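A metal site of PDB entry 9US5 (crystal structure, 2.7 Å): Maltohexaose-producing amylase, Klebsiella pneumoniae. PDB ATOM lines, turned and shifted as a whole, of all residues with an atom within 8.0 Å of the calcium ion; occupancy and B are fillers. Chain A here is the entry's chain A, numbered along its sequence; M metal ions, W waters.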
ATOM      1  N   MET A 194       9.065  15.679  -8.915  1.00  0.00           N
ATOM      2  CA  MET A 194       8.229  14.473  -9.136  1.00  0.00           C
ATOM      3  C   MET A 194       7.162  14.362  -8.042  1.00  0.00           C
ATOM      4  O   MET A 194       6.245  13.536  -8.204  1.00  0.00           O
ATOM      5  CB  MET A 194       9.087  13.200  -9.131  1.00  0.00           C
ATOM      6  CG  MET A 194       9.729  12.898 -10.466  1.00  0.00           C
ATOM      7  SD  MET A 194      10.557  11.285 -10.507  1.00  0.00           S
ATOM      8  CE  MET A 194       9.235  10.206  -9.948  1.00  0.00           C
ATOM      9  N   ASN A 195       7.273  15.164  -6.977  1.00  0.00           N
ATOM     10  CA  ASN A 195       6.429  15.050  -5.757  1.00  0.00           C
ATOM     11  C   ASN A 195       5.016  15.544  -6.037  1.00  0.00           C
ATOM     12  O   ASN A 195       4.065  14.869  -5.609  1.00  0.00           O
ATOM     13  CB  ASN A 195       7.003  15.840  -4.583  1.00  0.00           C
ATOM     14  CG  ASN A 195       6.067  15.778  -3.394  1.00  0.00           C
ATOM     15  OD1 ASN A 195       5.764  14.692  -2.906  1.00  0.00           O
ATOM     16  ND2 ASN A 195       5.567  16.934  -2.971  1.00  0.00           N
ATOM     17  N   HIS A 196       4.884  16.686  -6.713  1.00  0.00           N
ATOM     18  CA  HIS A 196       3.611  17.420  -6.889  1.00  0.00           C
ATOM     19  C   HIS A 196       3.535  18.046  -8.278  1.00  0.00           C
ATOM     20  O   HIS A 196       4.601  18.311  -8.878  1.00  0.00           O
ATOM     21  CB  HIS A 196       3.489  18.513  -5.809  1.00  0.00           C
ATOM     22  CG  HIS A 196       4.598  19.516  -5.890  1.00  0.00           C
ATOM     23  ND1 HIS A 196       5.728  19.416  -5.113  1.00  0.00           N
ATOM     24  CD2 HIS A 196       4.755  20.604  -6.676  1.00  0.00           C
ATOM     25  CE1 HIS A 196       6.546  20.411  -5.412  1.00  0.00           C
ATOM     26  NE2 HIS A 196       5.971  21.156  -6.372  1.00  0.00           N
ATOM     27  N   ARG A 264      -3.246  12.557  -5.030  1.00  0.00           N
ATOM     28  CA  ARG A 264      -3.958  12.761  -3.743  1.00  0.00           C
ATOM     29  C   ARG A 264      -4.165  14.269  -3.553  1.00  0.00           C
ATOM     30  O   ARG A 264      -3.182  15.025  -3.662  1.00  0.00           O
ATOM     31  CB  ARG A 264      -3.142  12.205  -2.580  1.00  0.00           C
ATOM     32  CG  ARG A 264      -3.256  10.693  -2.408  1.00  0.00           C
ATOM     33  CD  ARG A 264      -2.274  10.219  -1.367  1.00  0.00           C
ATOM     34  NE  ARG A 264      -0.906  10.478  -1.791  1.00  0.00           N
ATOM     35  CZ  ARG A 264      -0.139   9.626  -2.465  1.00  0.00           C
ATOM     36  NH1 ARG A 264       1.091   9.972  -2.810  1.00  0.00           N
ATOM     37  NH2 ARG A 264      -0.598   8.419  -2.795  1.00  0.00           N
ATOM     38  N   ASP A 276       1.882  11.029   6.384  1.00  0.00           N
ATOM     39  CA  ASP A 276       3.363  10.898   6.368  1.00  0.00           C
ATOM     40  C   ASP A 276       3.959  11.767   5.244  1.00  0.00           C
ATOM     41  O   ASP A 276       3.176  12.253   4.401  1.00  0.00           O
ATOM     42  CB  ASP A 276       3.811   9.434   6.277  1.00  0.00           C
ATOM     43  CG  ASP A 276       3.413   8.696   4.999  1.00  0.00           C
ATOM     44  OD1 ASP A 276       2.257   8.841   4.562  1.00  0.00           O
ATOM     45  OD2 ASP A 276       4.280   7.965   4.458  1.00  0.00           O
ATOM     46  N   ASP A 277       5.283  11.937   5.253  1.00  0.00           N
ATOM     47  CA  ASP A 277       6.061  12.809   4.320  1.00  0.00           C
ATOM     48  C   ASP A 277       5.769  12.426   2.858  1.00  0.00           C
ATOM     49  O   ASP A 277       5.672  13.355   2.020  1.00  0.00           O
ATOM     50  CB  ASP A 277       7.562  12.717   4.590  1.00  0.00           C
ATOM     51  CG  ASP A 277       8.020  13.348   5.902  1.00  0.00           C
ATOM     52  OD1 ASP A 277       7.414  14.360   6.312  1.00  0.00           O
ATOM     53  OD2 ASP A 277       8.975  12.817   6.505  1.00  0.00           O
ATOM     54  N   LEU A 278       5.628  11.126   2.565  1.00  0.00           N
ATOM     55  CA  LEU A 278       5.514  10.564   1.193  1.00  0.00           C
ATOM     56  C   LEU A 278       4.147  10.920   0.569  1.00  0.00           C
ATOM     57  O   LEU A 278       4.136  11.304  -0.613  1.00  0.00           O
ATOM     58  CB  LEU A 278       5.719   9.050   1.253  1.00  0.00           C
ATOM     59  CG  LEU A 278       7.163   8.567   1.092  1.00  0.00           C
ATOM     60  CD1 LEU A 278       8.137   9.372   1.935  1.00  0.00           C
ATOM     61  CD2 LEU A 278       7.284   7.092   1.423  1.00  0.00           C
ATOM     62  N   THR A 279       3.052  10.814   1.333  1.00  0.00           N
ATOM     63  CA  THR A 279       1.661  10.860   0.797  1.00  0.00           C
ATOM     64  C   THR A 279       0.915  12.135   1.249  1.00  0.00           C
ATOM     65  O   THR A 279      -0.258  12.278   0.859  1.00  0.00           O
ATOM     66  CB  THR A 279       0.891   9.585   1.175  1.00  0.00           C
ATOM     67  OG1 THR A 279       0.676   9.576   2.591  1.00  0.00           O
ATOM     68  CG2 THR A 279       1.602   8.321   0.770  1.00  0.00           C
ATOM     69  N   MET A 280       1.548  13.033   2.019  1.00  0.00           N
ATOM     70  CA  MET A 280       0.934  14.319   2.452  1.00  0.00           C
ATOM     71  C   MET A 280       0.914  15.292   1.264  1.00  0.00           C
ATOM     72  O   MET A 280       1.659  15.063   0.295  1.00  0.00           O
ATOM     73  CB  MET A 280       1.691  14.962   3.619  1.00  0.00           C
ATOM     74  CG  MET A 280       3.101  15.426   3.289  1.00  0.00           C
ATOM     75  SD  MET A 280       3.807  16.523   4.548  1.00  0.00           S
ATOM     76  CE  MET A 280       3.681  15.458   5.986  1.00  0.00           C
ATOM     77  N   SER A 281       0.091  16.348   1.338  1.00  0.00           N
ATOM     78  CA  SER A 281      -0.006  17.426   0.331  1.00  0.00           C
ATOM     79  C   SER A 281       0.717  18.676   0.828  1.00  0.00           C
ATOM     80  O   SER A 281       0.247  19.277   1.816  1.00  0.00           O
ATOM     81  CB  SER A 281      -1.448  17.732  -0.006  1.00  0.00           C
ATOM     82  OG  SER A 281      -1.536  18.907  -0.790  1.00  0.00           O
ATOM     83  N   LEU A 282       1.824  19.050   0.176  1.00  0.00           N
ATOM     84  CA  LEU A 282       2.612  20.279   0.495  1.00  0.00           C
ATOM     85  C   LEU A 282       1.854  21.514   0.002  1.00  0.00           C
ATOM     86  O   LEU A 282       1.744  21.679  -1.228  1.00  0.00           O
ATOM     87  CB  LEU A 282       3.996  20.188  -0.155  1.00  0.00           C
ATOM     88  CG  LEU A 282       5.044  19.365   0.588  1.00  0.00           C
ATOM     89  CD1 LEU A 282       4.705  17.883   0.566  1.00  0.00           C
ATOM     90  CD2 LEU A 282       6.429  19.609   0.007  1.00  0.00           C
ATOM     91  N   PRO A 286      -1.463  19.313  -5.526  1.00  0.00           N
ATOM     92  CA  PRO A 286      -1.762  17.920  -5.835  1.00  0.00           C
ATOM     93  C   PRO A 286      -0.495  17.075  -5.632  1.00  0.00           C
ATOM     94  O   PRO A 286       0.520  17.402  -6.221  1.00  0.00           O
ATOM     95  CB  PRO A 286      -2.226  17.948  -7.306  1.00  0.00           C
ATOM     96  CG  PRO A 286      -1.740  19.274  -7.847  1.00  0.00           C
ATOM     97  CD  PRO A 286      -1.739  20.212  -6.655  1.00  0.00           C
ATOM     98  N   ASP A 287      -0.585  16.058  -4.773  1.00  0.00           N
ATOM     99  CA  ASP A 287       0.515  15.108  -4.474  1.00  0.00           C
ATOM    100  C   ASP A 287       0.448  13.956  -5.475  1.00  0.00           C
ATOM    101  O   ASP A 287      -0.564  13.237  -5.480  1.00  0.00           O
ATOM    102  CB  ASP A 287       0.436  14.607  -3.023  1.00  0.00           C
ATOM    103  CG  ASP A 287       1.616  13.734  -2.636  1.00  0.00           C
ATOM    104  OD1 ASP A 287       2.769  14.218  -2.751  1.00  0.00           O
ATOM    105  OD2 ASP A 287       1.392  12.574  -2.249  1.00  0.00           O
ATOM    106  N   LEU A 288       1.482  13.785  -6.300  1.00  0.00           N
ATOM    107  CA  LEU A 288       1.561  12.745  -7.347  1.00  0.00           C
ATOM    108  C   LEU A 288       1.724  11.377  -6.668  1.00  0.00           C
ATOM    109  O   LEU A 288       2.572  11.277  -5.781  1.00  0.00           O
ATOM    110  CB  LEU A 288       2.720  13.064  -8.292  1.00  0.00           C
ATOM    111  CG  LEU A 288       2.493  14.291  -9.173  1.00  0.00           C
ATOM    112  CD1 LEU A 288       3.801  14.857  -9.684  1.00  0.00           C
ATOM    113  CD2 LEU A 288       1.559  13.950 -10.329  1.00  0.00           C
ATOM    114  N   LYS A 289       0.918  10.399  -7.066  1.00  0.00           N
ATOM    115  CA  LYS A 289       0.875   9.041  -6.466  1.00  0.00           C
ATOM    116  C   LYS A 289       2.054   8.253  -7.048  1.00  0.00           C
ATOM    117  O   LYS A 289       1.827   7.368  -7.896  1.00  0.00           O
ATOM    118  CB  LYS A 289      -0.493   8.394  -6.700  1.00  0.00           C
ATOM    119  CG  LYS A 289      -1.649   9.157  -6.075  1.00  0.00           C
ATOM    120  CD  LYS A 289      -3.026   8.666  -6.467  1.00  0.00           C
ATOM    121  CE  LYS A 289      -3.316   7.283  -5.943  1.00  0.00           C
ATOM    122  NZ  LYS A 289      -4.773   7.070  -5.783  1.00  0.00           N
ATOM    123  N   THR A 290       3.271   8.600  -6.620  1.00  0.00           N
ATOM    124  CA  THR A 290       4.545   8.051  -7.140  1.00  0.00           C
ATOM    125  C   THR A 290       4.735   6.606  -6.649  1.00  0.00           C
ATOM    126  O   THR A 290       5.506   5.871  -7.288  1.00  0.00           O
ATOM    127  CB  THR A 290       5.726   8.937  -6.734  1.00  0.00           C
ATOM    128  OG1 THR A 290       5.746   8.974  -5.305  1.00  0.00           O
ATOM    129  CG2 THR A 290       5.633  10.340  -7.294  1.00  0.00           C
ATOM    130  N   GLU A 291       4.090   6.233  -5.539  1.00  0.00           N
ATOM    131  CA  GLU A 291       4.207   4.886  -4.899  1.00  0.00           C
ATOM    132  C   GLU A 291       3.188   3.912  -5.515  1.00  0.00           C
ATOM    133  O   GLU A 291       3.416   2.700  -5.397  1.00  0.00           O
ATOM    134  CB  GLU A 291       4.043   4.994  -3.373  1.00  0.00           C
ATOM    135  CG  GLU A 291       2.598   4.977  -2.886  1.00  0.00           C
ATOM    136  CD  GLU A 291       1.711   6.121  -3.345  1.00  0.00           C
ATOM    137  OE1 GLU A 291       2.233   7.238  -3.554  1.00  0.00           O
ATOM    138  OE2 GLU A 291       0.488   5.894  -3.509  1.00  0.00           O
ATOM    139  N   THR A 342      12.304  18.360  -3.232  1.00  0.00           N
ATOM    140  CA  THR A 342      11.457  17.662  -2.217  1.00  0.00           C
ATOM    141  C   THR A 342      11.727  16.146  -2.236  1.00  0.00           C
ATOM    142  O   THR A 342      10.771  15.366  -2.398  1.00  0.00           O
ATOM    143  CB  THR A 342       9.978  18.054  -2.419  1.00  0.00           C
ATOM    144  OG1 THR A 342       9.673  18.114  -3.813  1.00  0.00           O
ATOM    145  CG2 THR A 342       9.642  19.387  -1.793  1.00  0.00           C
ATOM    146  N   LYS A 344      12.557  14.119   0.188  1.00  0.00           N
ATOM    147  CA  LYS A 344      12.069  13.356   1.381  1.00  0.00           C
ATOM    148  C   LYS A 344      10.573  13.012   1.221  1.00  0.00           C
ATOM    149  O   LYS A 344      10.103  12.147   1.989  1.00  0.00           O
ATOM    150  CB  LYS A 344      12.345  14.100   2.683  1.00  0.00           C
ATOM    151  CG  LYS A 344      11.781  15.506   2.787  1.00  0.00           C
ATOM    152  CD  LYS A 344      11.385  15.926   4.195  1.00  0.00           C
ATOM    153  CE  LYS A 344      12.569  16.116   5.129  1.00  0.00           C
ATOM    154  NZ  LYS A 344      12.172  16.838   6.358  1.00  0.00           N
ATOM    155  N   HIS A 345       9.867  13.643   0.269  1.00  0.00           N
ATOM    156  CA  HIS A 345       8.397  13.514   0.098  1.00  0.00           C
ATOM    157  C   HIS A 345       8.061  12.500  -1.012  1.00  0.00           C
ATOM    158  O   HIS A 345       6.872  12.424  -1.410  1.00  0.00           O
ATOM    159  CB  HIS A 345       7.777  14.897  -0.142  1.00  0.00           C
ATOM    160  CG  HIS A 345       7.929  15.822   1.020  1.00  0.00           C
ATOM    161  ND1 HIS A 345       8.678  16.983   0.949  1.00  0.00           N
ATOM    162  CD2 HIS A 345       7.438  15.764   2.275  1.00  0.00           C
ATOM    163  CE1 HIS A 345       8.644  17.599   2.108  1.00  0.00           C
ATOM    164  NE2 HIS A 345       7.881  16.871   2.937  1.00  0.00           N
ATOM    165  N   VAL A 346       9.046  11.740  -1.468  1.00  0.00           N
ATOM    166  CA  VAL A 346       8.939  10.708  -2.548  1.00  0.00           C
ATOM    167  C   VAL A 346       9.809   9.522  -2.143  1.00  0.00           C
ATOM    168  O   VAL A 346      10.986   9.746  -1.813  1.00  0.00           O
ATOM    169  CB  VAL A 346       9.404  11.293  -3.899  1.00  0.00           C
ATOM    170  CG1 VAL A 346       9.589  10.224  -4.958  1.00  0.00           C
ATOM    171  CG2 VAL A 346       8.465  12.387  -4.402  1.00  0.00           C
ATOM    172  N   GLU A 347       9.249   8.305  -2.174  1.00  0.00           N
ATOM    173  CA  GLU A 347       9.938   7.026  -1.823  1.00  0.00           C
ATOM    174  C   GLU A 347      11.257   6.917  -2.598  1.00  0.00           C
ATOM    175  O   GLU A 347      11.387   7.551  -3.662  1.00  0.00           O
ATOM    176  CB  GLU A 347       9.003   5.832  -2.055  1.00  0.00           C
ATOM    177  CG  GLU A 347       8.545   5.640  -3.496  1.00  0.00           C
ATOM    178  CD  GLU A 347       7.461   6.568  -4.037  1.00  0.00           C
ATOM    179  OE1 GLU A 347       6.730   7.188  -3.224  1.00  0.00           O
ATOM    180  OE2 GLU A 347       7.341   6.670  -5.273  1.00  0.00           O
HETATM  181 CA    CA M   1       4.542  12.761  -2.112  1.00  0.00          CA
HETATM  182  O   HOH W   1       4.405  12.517  -4.494  1.00  0.00           O
HETATM  183  O   HOH W   2       4.168  14.364  -0.232  1.00  0.00           O
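OD2 of Asp 287 is in salt-bridge range of NH1 of Arg 264, at 2.7 Å.
O of Asn 195 is in hydrogen-bond range of N of Leu 288 (2.9 Å).
ND1 of His 196 lies within hydrogen-bond range of ND2 of Asn 195, at 3.3 Å.
Within 4 Å of the calcium ion: Asn 195, Leu 278, Asp 287 and His 345.
The nearest printed residue that does not touch the calcium ion is Thr 279 (4.2 Å).
The calcium ion is bound by O of Leu 278 (2.1 Å), OD1 of Asp 287 (2.4 Å), water W1 (2.4 Å), OD1 of Asn 195 (2.4 Å), O of His 345 (2.5 Å) and water W2 (2.5 Å).
Water W1 lies within hydrogen-bond range of O of Leu 288 and O of Asn 195.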
